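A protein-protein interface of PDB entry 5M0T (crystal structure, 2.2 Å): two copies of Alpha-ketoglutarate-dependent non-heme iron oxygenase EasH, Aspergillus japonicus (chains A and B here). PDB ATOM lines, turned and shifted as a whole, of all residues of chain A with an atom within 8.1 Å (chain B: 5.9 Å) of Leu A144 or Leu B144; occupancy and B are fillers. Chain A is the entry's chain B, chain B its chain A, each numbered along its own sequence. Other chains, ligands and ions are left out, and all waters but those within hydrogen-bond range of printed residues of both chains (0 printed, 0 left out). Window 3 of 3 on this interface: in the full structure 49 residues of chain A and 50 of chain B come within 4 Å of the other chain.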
ATOM      1  N   HIS A 135      19.390  -3.915  21.840  1.00  0.00           N
ATOM      2  CA  HIS A 135      20.130  -4.508  20.704  1.00  0.00           C
ATOM      3  C   HIS A 135      21.347  -3.688  20.233  1.00  0.00           C
ATOM      4  O   HIS A 135      22.124  -4.162  19.410  1.00  0.00           O
ATOM      5  CB  HIS A 135      19.193  -4.898  19.546  1.00  0.00           C
ATOM      6  CG  HIS A 135      18.848  -3.793  18.581  1.00  0.00           C
ATOM      7  ND1 HIS A 135      18.131  -4.042  17.422  1.00  0.00           N
ATOM      8  CD2 HIS A 135      19.138  -2.464  18.567  1.00  0.00           C
ATOM      9  CE1 HIS A 135      17.996  -2.916  16.742  1.00  0.00           C
ATOM     10  NE2 HIS A 135      18.587  -1.943  17.418  1.00  0.00           N
ATOM     11  N   ASP A 136      21.518  -2.474  20.764  1.00  0.00           N
ATOM     12  CA  ASP A 136      22.722  -1.688  20.466  1.00  0.00           C
ATOM     13  C   ASP A 136      24.018  -2.251  21.077  1.00  0.00           C
ATOM     14  O   ASP A 136      25.087  -1.773  20.771  1.00  0.00           O
ATOM     15  CB  ASP A 136      22.514  -0.201  20.793  1.00  0.00           C
ATOM     16  CG  ASP A 136      21.508   0.471  19.821  1.00  0.00           C
ATOM     17  OD1 ASP A 136      21.567   0.231  18.594  1.00  0.00           O
ATOM     18  OD2 ASP A 136      20.649   1.251  20.271  1.00  0.00           O
ATOM     19  N   ILE A 138      24.925  -5.151  20.094  1.00  0.00           N
ATOM     20  CA  ILE A 138      25.367  -5.946  18.954  1.00  0.00           C
ATOM     21  C   ILE A 138      25.555  -5.029  17.744  1.00  0.00           C
ATOM     22  O   ILE A 138      24.577  -4.449  17.283  1.00  0.00           O
ATOM     23  CB  ILE A 138      24.313  -7.022  18.611  1.00  0.00           C
ATOM     24  CG1 ILE A 138      24.110  -7.977  19.787  1.00  0.00           C
ATOM     25  CG2 ILE A 138      24.707  -7.801  17.356  1.00  0.00           C
ATOM     26  CD1 ILE A 138      22.793  -8.732  19.699  1.00  0.00           C
ATOM     27  N   PRO A 139      26.795  -4.902  17.210  1.00  0.00           N
ATOM     28  CA  PRO A 139      27.015  -3.887  16.154  1.00  0.00           C
ATOM     29  C   PRO A 139      26.183  -4.024  14.860  1.00  0.00           C
ATOM     30  O   PRO A 139      25.734  -3.026  14.321  1.00  0.00           O
ATOM     31  CB  PRO A 139      28.517  -4.014  15.843  1.00  0.00           C
ATOM     32  CG  PRO A 139      29.109  -4.581  17.082  1.00  0.00           C
ATOM     33  CD  PRO A 139      28.069  -5.477  17.684  1.00  0.00           C
ATOM     34  N   ILE A 140      26.009  -5.235  14.352  1.00  0.00           N
ATOM     35  CA  ILE A 140      25.165  -5.445  13.172  1.00  0.00           C
ATOM     36  C   ILE A 140      23.709  -4.994  13.407  1.00  0.00           C
ATOM     37  O   ILE A 140      23.094  -4.462  12.506  1.00  0.00           O
ATOM     38  CB  ILE A 140      25.241  -6.903  12.651  1.00  0.00           C
ATOM     39  CG1 ILE A 140      24.488  -7.083  11.320  1.00  0.00           C
ATOM     40  CG2 ILE A 140      24.661  -7.897  13.645  1.00  0.00           C
ATOM     41  CD1 ILE A 140      24.822  -6.071  10.241  1.00  0.00           C
ATOM     42  N   CYS A 141      23.182  -5.158  14.611  1.00  0.00           N
ATOM     43  CA  CYS A 141      21.823  -4.691  14.928  1.00  0.00           C
ATOM     44  C   CYS A 141      21.696  -3.163  14.995  1.00  0.00           C
ATOM     45  O   CYS A 141      20.661  -2.600  14.635  1.00  0.00           O
ATOM     46  CB  CYS A 141      21.314  -5.297  16.233  1.00  0.00           C
ATOM     47  SG  CYS A 141      21.110  -7.107  16.201  1.00  0.00           S
ATOM     48  N   THR A 142      22.741  -2.496  15.467  1.00  0.00           N
ATOM     49  CA  THR A 142      22.808  -1.030  15.451  1.00  0.00           C
ATOM     50  C   THR A 142      22.801  -0.495  14.031  1.00  0.00           C
ATOM     51  O   THR A 142      22.149   0.496  13.742  1.00  0.00           O
ATOM     52  CB  THR A 142      24.080  -0.547  16.175  1.00  0.00           C
ATOM     53  OG1 THR A 142      24.033  -1.015  17.526  1.00  0.00           O
ATOM     54  CG2 THR A 142      24.207   0.970  16.160  1.00  0.00           C
ATOM     55  N   THR A 143      23.528  -1.162  13.145  1.00  0.00           N
ATOM     56  CA  THR A 143      23.591  -0.767  11.737  1.00  0.00           C
ATOM     57  C   THR A 143      22.246  -0.903  11.021  1.00  0.00           C
ATOM     58  O   THR A 143      21.858  -0.040  10.254  1.00  0.00           O
ATOM     59  CB  THR A 143      24.659  -1.606  11.025  1.00  0.00           C
ATOM     60  OG1 THR A 143      25.933  -1.285  11.613  1.00  0.00           O
ATOM     61  CG2 THR A 143      24.690  -1.339   9.503  1.00  0.00           C
ATOM     62  N   LEU A 144      21.562  -2.006  11.286  1.00  0.00           N
ATOM     63  CA  LEU A 144      20.260  -2.317  10.677  1.00  0.00           C
ATOM     64  C   LEU A 144      19.091  -1.530  11.257  1.00  0.00           C
ATOM     65  O   LEU A 144      18.160  -1.241  10.541  1.00  0.00           O
ATOM     66  CB  LEU A 144      19.981  -3.833  10.766  1.00  0.00           C
ATOM     67  CG  LEU A 144      20.978  -4.704   9.982  1.00  0.00           C
ATOM     68  CD1 LEU A 144      20.733  -6.187  10.239  1.00  0.00           C
ATOM     69  CD2 LEU A 144      20.965  -4.400   8.495  1.00  0.00           C
ATOM     70  N   GLY A 145      19.132  -1.181  12.540  1.00  0.00           N
ATOM     71  CA  GLY A 145      18.063  -0.399  13.155  1.00  0.00           C
ATOM     72  C   GLY A 145      16.741  -1.171  13.161  1.00  0.00           C
ATOM     73  O   GLY A 145      16.697  -2.315  13.618  1.00  0.00           O
ATOM     74  N   ARG A 146      15.676  -0.547  12.653  1.00  0.00           N
ATOM     75  CA  ARG A 146      14.376  -1.193  12.557  1.00  0.00           C
ATOM     76  C   ARG A 146      14.410  -2.474  11.738  1.00  0.00           C
ATOM     77  O   ARG A 146      13.704  -3.414  12.077  1.00  0.00           O
ATOM     78  CB  ARG A 146      13.322  -0.272  11.955  1.00  0.00           C
ATOM     79  CG  ARG A 146      11.947  -0.925  11.974  1.00  0.00           C
ATOM     80  CD  ARG A 146      10.797  -0.012  11.697  1.00  0.00           C
ATOM     81  NE  ARG A 146       9.762  -0.633  10.877  1.00  0.00           N
ATOM     82  CZ  ARG A 146       9.105  -1.765  11.156  1.00  0.00           C
ATOM     83  NH1 ARG A 146       9.374  -2.484  12.242  1.00  0.00           N
ATOM     84  NH2 ARG A 146       8.174  -2.206  10.309  1.00  0.00           N
ATOM     85  N   GLN A 147      15.237  -2.525  10.695  1.00  0.00           N
ATOM     86  CA  GLN A 147      15.310  -3.709   9.823  1.00  0.00           C
ATOM     87  C   GLN A 147      16.045  -4.895  10.443  1.00  0.00           C
ATOM     88  O   GLN A 147      16.152  -5.945   9.809  1.00  0.00           O
ATOM     89  CB  GLN A 147      15.948  -3.359   8.466  1.00  0.00           C
ATOM     90  CG  GLN A 147      14.963  -2.754   7.479  1.00  0.00           C
ATOM     91  CD  GLN A 147      14.424  -1.419   7.943  1.00  0.00           C
ATOM     92  OE1 GLN A 147      13.226  -1.264   8.155  1.00  0.00           O
ATOM     93  NE2 GLN A 147      15.317  -0.448   8.121  1.00  0.00           N
ATOM     94  N   SER A 148      16.572  -4.722  11.653  1.00  0.00           N
ATOM     95  CA  SER A 148      17.263  -5.788  12.333  1.00  0.00           C
ATOM     96  C   SER A 148      16.341  -6.961  12.651  1.00  0.00           C
ATOM     97  O   SER A 148      15.188  -6.759  13.006  1.00  0.00           O
ATOM     98  CB  SER A 148      17.855  -5.268  13.642  1.00  0.00           C
ATOM     99  OG  SER A 148      18.598  -6.277  14.305  1.00  0.00           O
ATOM    100  N   PRO A 149      16.858  -8.193  12.547  1.00  0.00           N
ATOM    101  CA  PRO A 149      16.111  -9.306  13.106  1.00  0.00           C
ATOM    102  C   PRO A 149      16.092  -9.198  14.625  1.00  0.00           C
ATOM    103  O   PRO A 149      16.948  -8.519  15.206  1.00  0.00           O
ATOM    104  CB  PRO A 149      16.946 -10.513  12.682  1.00  0.00           C
ATOM    105  CG  PRO A 149      18.326  -9.990  12.671  1.00  0.00           C
ATOM    106  CD  PRO A 149      18.176  -8.633  12.058  1.00  0.00           C
ATOM    107  N   GLU A 179      10.633   4.409  12.437  1.00  0.00           N
ATOM    108  CA  GLU A 179      11.406   4.254  11.209  1.00  0.00           C
ATOM    109  C   GLU A 179      12.914   4.374  11.462  1.00  0.00           C
ATOM    110  O   GLU A 179      13.686   3.506  11.040  1.00  0.00           O
ATOM    111  CB  GLU A 179      10.965   5.275  10.157  1.00  0.00           C
ATOM    112  CG  GLU A 179       9.521   5.159   9.697  1.00  0.00           C
ATOM    113  CD  GLU A 179       9.250   3.877   8.929  1.00  0.00           C
ATOM    114  OE1 GLU A 179       9.181   3.945   7.684  1.00  0.00           O
ATOM    115  OE2 GLU A 179       9.120   2.806   9.568  1.00  0.00           O
ATOM    116  N   ASP A 180      13.313   5.421  12.186  1.00  0.00           N
ATOM    117  CA  ASP A 180      14.728   5.773  12.375  1.00  0.00           C
ATOM    118  C   ASP A 180      15.218   5.468  13.798  1.00  0.00           C
ATOM    119  O   ASP A 180      14.960   6.229  14.727  1.00  0.00           O
ATOM    120  CB  ASP A 180      14.909   7.260  12.032  1.00  0.00           C
ATOM    121  CG  ASP A 180      16.358   7.713  12.065  1.00  0.00           C
ATOM    122  OD1 ASP A 180      17.284   6.876  12.147  1.00  0.00           O
ATOM    123  OD2 ASP A 180      16.568   8.938  12.001  1.00  0.00           O
ATOM    124  N   PHE A 181      15.938   4.366  13.960  1.00  0.00           N
ATOM    125  CA  PHE A 181      16.466   3.979  15.278  1.00  0.00           C
ATOM    126  C   PHE A 181      17.683   4.821  15.728  1.00  0.00           C
ATOM    127  O   PHE A 181      18.055   4.804  16.905  1.00  0.00           O
ATOM    128  CB  PHE A 181      16.816   2.474  15.290  1.00  0.00           C
ATOM    129  CG  PHE A 181      15.643   1.552  15.556  1.00  0.00           C
ATOM    130  CD1 PHE A 181      14.312   1.933  15.316  1.00  0.00           C
ATOM    131  CD2 PHE A 181      15.882   0.258  16.018  1.00  0.00           C
ATOM    132  CE1 PHE A 181      13.264   1.047  15.564  1.00  0.00           C
ATOM    133  CE2 PHE A 181      14.832  -0.626  16.259  1.00  0.00           C
ATOM    134  CZ  PHE A 181      13.523  -0.228  16.028  1.00  0.00           C
ATOM    135  N   SER A 182      18.313   5.533  14.800  1.00  0.00           N
ATOM    136  CA  SER A 182      19.456   6.375  15.124  1.00  0.00           C
ATOM    137  C   SER A 182      19.044   7.786  15.549  1.00  0.00           C
ATOM    138  O   SER A 182      19.897   8.560  15.985  1.00  0.00           O
ATOM    139  CB  SER A 182      20.397   6.454  13.920  1.00  0.00           C
ATOM    140  OG  SER A 182      19.830   7.241  12.896  1.00  0.00           O
ATOM    141  N   LYS A 207      14.530  -4.021  20.623  1.00  0.00           N
ATOM    142  CA  LYS A 207      14.220  -2.923  19.715  1.00  0.00           C
ATOM    143  C   LYS A 207      13.396  -1.838  20.368  1.00  0.00           C
ATOM    144  O   LYS A 207      13.121  -0.830  19.744  1.00  0.00           O
ATOM    145  CB  LYS A 207      13.480  -3.459  18.496  1.00  0.00           C
ATOM    146  CG  LYS A 207      14.340  -4.441  17.722  1.00  0.00           C
ATOM    147  CD  LYS A 207      13.645  -5.095  16.555  1.00  0.00           C
ATOM    148  CE  LYS A 207      13.854  -4.338  15.260  1.00  0.00           C
ATOM    149  NZ  LYS A 207      13.369  -5.164  14.138  1.00  0.00           N
ATOM    150  N   PHE A 234      24.500 -14.840  18.068  1.00  0.00           N
ATOM    151  CA  PHE A 234      25.235 -13.751  18.710  1.00  0.00           C
ATOM    152  C   PHE A 234      25.907 -14.158  20.030  1.00  0.00           C
ATOM    153  O   PHE A 234      25.296 -14.796  20.907  1.00  0.00           O
ATOM    154  CB  PHE A 234      24.331 -12.544  18.953  1.00  0.00           C
ATOM    155  CG  PHE A 234      23.728 -11.990  17.702  1.00  0.00           C
ATOM    156  CD1 PHE A 234      24.529 -11.433  16.714  1.00  0.00           C
ATOM    157  CD2 PHE A 234      22.349 -12.062  17.485  1.00  0.00           C
ATOM    158  CE1 PHE A 234      23.970 -10.930  15.546  1.00  0.00           C
ATOM    159  CE2 PHE A 234      21.784 -11.562  16.312  1.00  0.00           C
ATOM    160  CZ  PHE A 234      22.598 -10.995  15.342  1.00  0.00           C
ATOM    161  N   HIS B 135      30.038 -17.540   5.088  1.00  0.00           N
ATOM    162  CA  HIS B 135      29.159 -16.772   5.984  1.00  0.00           C
ATOM    163  C   HIS B 135      27.718 -17.289   6.078  1.00  0.00           C
ATOM    164  O   HIS B 135      26.950 -16.824   6.914  1.00  0.00           O
ATOM    165  CB  HIS B 135      29.230 -15.253   5.687  1.00  0.00           C
ATOM    166  CG  HIS B 135      28.327 -14.757   4.597  1.00  0.00           C
ATOM    167  ND1 HIS B 135      28.170 -13.410   4.343  1.00  0.00           N
ATOM    168  CD2 HIS B 135      27.507 -15.397   3.724  1.00  0.00           C
ATOM    169  CE1 HIS B 135      27.296 -13.250   3.365  1.00  0.00           C
ATOM    170  NE2 HIS B 135      26.883 -14.439   2.973  1.00  0.00           N
ATOM    171  N   PRO B 139      22.974 -17.027  10.302  1.00  0.00           N
ATOM    172  CA  PRO B 139      21.701 -16.690   9.620  1.00  0.00           C
ATOM    173  C   PRO B 139      21.499 -15.207   9.207  1.00  0.00           C
ATOM    174  O   PRO B 139      20.966 -14.948   8.141  1.00  0.00           O
ATOM    175  CB  PRO B 139      20.632 -17.107  10.636  1.00  0.00           C
ATOM    176  CG  PRO B 139      21.281 -18.143  11.463  1.00  0.00           C
ATOM    177  CD  PRO B 139      22.736 -17.778  11.546  1.00  0.00           C
ATOM    178  N   ILE B 140      21.890 -14.258  10.049  1.00  0.00           N
ATOM    179  CA  ILE B 140      21.790 -12.843   9.678  1.00  0.00           C
ATOM    180  C   ILE B 140      22.631 -12.512   8.431  1.00  0.00           C
ATOM    181  O   ILE B 140      22.210 -11.704   7.621  1.00  0.00           O
ATOM    182  CB  ILE B 140      22.129 -11.896  10.868  1.00  0.00           C
ATOM    183  CG1 ILE B 140      21.888 -10.416  10.526  1.00  0.00           C
ATOM    184  CG2 ILE B 140      23.581 -12.027  11.303  1.00  0.00           C
ATOM    185  CD1 ILE B 140      20.545 -10.100   9.922  1.00  0.00           C
ATOM    186  N   CYS B 141      23.781 -13.155   8.254  1.00  0.00           N
ATOM    187  CA  CYS B 141      24.602 -12.940   7.053  1.00  0.00           C
ATOM    188  C   CYS B 141      23.985 -13.524   5.774  1.00  0.00           C
ATOM    189  O   CYS B 141      24.156 -12.967   4.695  1.00  0.00           O
ATOM    190  CB  CYS B 141      26.008 -13.515   7.236  1.00  0.00           C
ATOM    191  SG  CYS B 141      27.015 -12.711   8.495  1.00  0.00           S
ATOM    192  N   THR B 142      23.289 -14.648   5.899  1.00  0.00           N
ATOM    193  CA  THR B 142      22.529 -15.226   4.795  1.00  0.00           C
ATOM    194  C   THR B 142      21.414 -14.299   4.348  1.00  0.00           C
ATOM    195  O   THR B 142      21.172 -14.148   3.160  1.00  0.00           O
ATOM    196  CB  THR B 142      21.937 -16.591   5.202  1.00  0.00           C
ATOM    197  OG1 THR B 142      23.006 -17.474   5.548  1.00  0.00           O
ATOM    198  CG2 THR B 142      21.119 -17.218   4.074  1.00  0.00           C
ATOM    199  N   THR B 143      20.743 -13.680   5.299  1.00  0.00           N
ATOM    200  CA  THR B 143      19.653 -12.744   5.006  1.00  0.00           C
ATOM    201  C   THR B 143      20.137 -11.491   4.266  1.00  0.00           C
ATOM    202  O   THR B 143      19.500 -11.035   3.316  1.00  0.00           O
ATOM    203  CB  THR B 143      18.963 -12.329   6.317  1.00  0.00           C
ATOM    204  OG1 THR B 143      18.390 -13.493   6.917  1.00  0.00           O
ATOM    205  CG2 THR B 143      17.875 -11.267   6.082  1.00  0.00           C
ATOM    206  N   LEU B 144      21.266 -10.952   4.726  1.00  0.00           N
ATOM    207  CA  LEU B 144      21.861  -9.740   4.161  1.00  0.00           C
ATOM    208  C   LEU B 144      22.582  -9.950   2.830  1.00  0.00           C
ATOM    209  O   LEU B 144      22.599  -9.047   2.012  1.00  0.00           O
ATOM    210  CB  LEU B 144      22.805  -9.093   5.181  1.00  0.00           C
ATOM    211  CG  LEU B 144      22.112  -8.591   6.465  1.00  0.00           C
ATOM    212  CD1 LEU B 144      23.131  -8.117   7.501  1.00  0.00           C
ATOM    213  CD2 LEU B 144      21.093  -7.495   6.148  1.00  0.00           C
ATOM    214  N   GLY B 145      23.166 -11.123   2.607  1.00  0.00           N
ATOM    215  CA  GLY B 145      23.867 -11.386   1.372  1.00  0.00           C
ATOM    216  C   GLY B 145      25.083 -10.478   1.183  1.00  0.00           C
ATOM    217  O   GLY B 145      25.923 -10.387   2.058  1.00  0.00           O
ATOM    218  N   ARG B 146      25.161  -9.806   0.036  1.00  0.00           N
ATOM    219  CA  ARG B 146      26.232  -8.868  -0.249  1.00  0.00           C
ATOM    220  C   ARG B 146      26.315  -7.743   0.763  1.00  0.00           C
ATOM    221  O   ARG B 146      27.405  -7.305   1.074  1.00  0.00           O
ATOM    222  CB  ARG B 146      26.098  -8.248  -1.636  1.00  0.00           C
ATOM    223  CG  ARG B 146      27.327  -7.414  -1.976  1.00  0.00           C
ATOM    224  CD  ARG B 146      27.303  -6.930  -3.398  1.00  0.00           C
ATOM    225  NE  ARG B 146      26.181  -6.002  -3.583  1.00  0.00           N
ATOM    226  CZ  ARG B 146      25.944  -5.284  -4.685  1.00  0.00           C
ATOM    227  NH1 ARG B 146      26.751  -5.350  -5.747  1.00  0.00           N
ATOM    228  NH2 ARG B 146      24.894  -4.476  -4.719  1.00  0.00           N
ATOM    229  N   GLN B 147      25.176  -7.289   1.283  1.00  0.00           N
ATOM    230  CA  GLN B 147      25.151  -6.178   2.250  1.00  0.00           C
ATOM    231  C   GLN B 147      25.614  -6.564   3.649  1.00  0.00           C
ATOM    232  O   GLN B 147      25.666  -5.716   4.542  1.00  0.00           O
ATOM    233  CB  GLN B 147      23.757  -5.528   2.327  1.00  0.00           C
ATOM    234  CG  GLN B 147      23.516  -4.505   1.228  1.00  0.00           C
ATOM    235  CD  GLN B 147      23.525  -5.126  -0.158  1.00  0.00           C
ATOM    236  OE1 GLN B 147      24.360  -4.797  -0.999  1.00  0.00           O
ATOM    237  NE2 GLN B 147      22.603  -6.057  -0.388  1.00  0.00           N
ATOM    238  N   SER B 148      25.934  -7.835   3.849  1.00  0.00           N
ATOM    239  CA  SER B 148      26.408  -8.312   5.126  1.00  0.00           C
ATOM    240  C   SER B 148      27.743  -7.671   5.496  1.00  0.00           C
ATOM    241  O   SER B 148      28.593  -7.455   4.627  1.00  0.00           O
ATOM    242  CB  SER B 148      26.587  -9.820   5.075  1.00  0.00           C
ATOM    243  OG  SER B 148      27.023 -10.323   6.318  1.00  0.00           O
ATOM    244  N   PRO B 149      27.945  -7.384   6.792  1.00  0.00           N
ATOM    245  CA  PRO B 149      29.280  -7.049   7.206  1.00  0.00           C
ATOM    246  C   PRO B 149      30.190  -8.261   7.078  1.00  0.00           C
ATOM    247  O   PRO B 149      29.700  -9.394   7.052  1.00  0.00           O
ATOM    248  CB  PRO B 149      29.103  -6.654   8.668  1.00  0.00           C
ATOM    249  CG  PRO B 149      28.003  -7.551   9.109  1.00  0.00           C
ATOM    250  CD  PRO B 149      27.044  -7.496   7.945  1.00  0.00           C
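Of the 20 printed residues of chain A, 3 touch a printed residue of chain B.
Hydrophobic or aromatic side chains of chain A within 4 Å of the printed part of chain B: Ile A140, Leu A144 and Pro A149.
Among the printed residues, no Asp or Glu carboxylate lies within 4 Å of a Lys or Arg side-chain nitrogen of the other chain.
Of chain B, only Ile B140 and Leu B144 come within 4 Å of Leu A144.
Printed residues of chain A within 4 Å of Leu B144: Ile A140 (3.8 Å) and Leu A144 (3.9 Å).
No residue of chain A comes within 4 Å of Gly B145.
Printed residues of chain B within 4 Å of Ile A140: Leu B144 (3.8 Å) and Pro B149 (3.5 Å).
Printed residues of chain A within 4 Å of Ile B140: Leu A144 (3.9 Å) and Pro A149 (3.5 Å).
Of the printed residues of chain B, Pro A149 touches Ile B140 (3.5 Å).
Printed residues of chain A within 4 Å of Pro B149: Ile A140.
The nearest printed residue of chain B that does not touch Leu A144 is Gln B147 (6.3 Å).
Ile A140 touches Leu B144, and with the chains exchanged Leu A144 touches Ile B140.
Ile A140 touches Pro B149, and with the chains exchanged Pro A149 touches Ile B140.
Leu A144 touches its own counterpart, Leu B144.
Positions printed for both chains: 135, 139, 140, 141, 142, 143, 144, 145, 146, 147, 148 and 149.
CD1 of Ile A140 touches CD1 of Leu B144, at 3.8 Å.
Ile A140 touches Pro B149 (CD1 to CD, 3.5 Å).
Leu A144 touches Ile B140.
Leu B144 touches Leu A144.
Pro A149 touches Ile B140 (CD to CD1, 3.5 Å).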
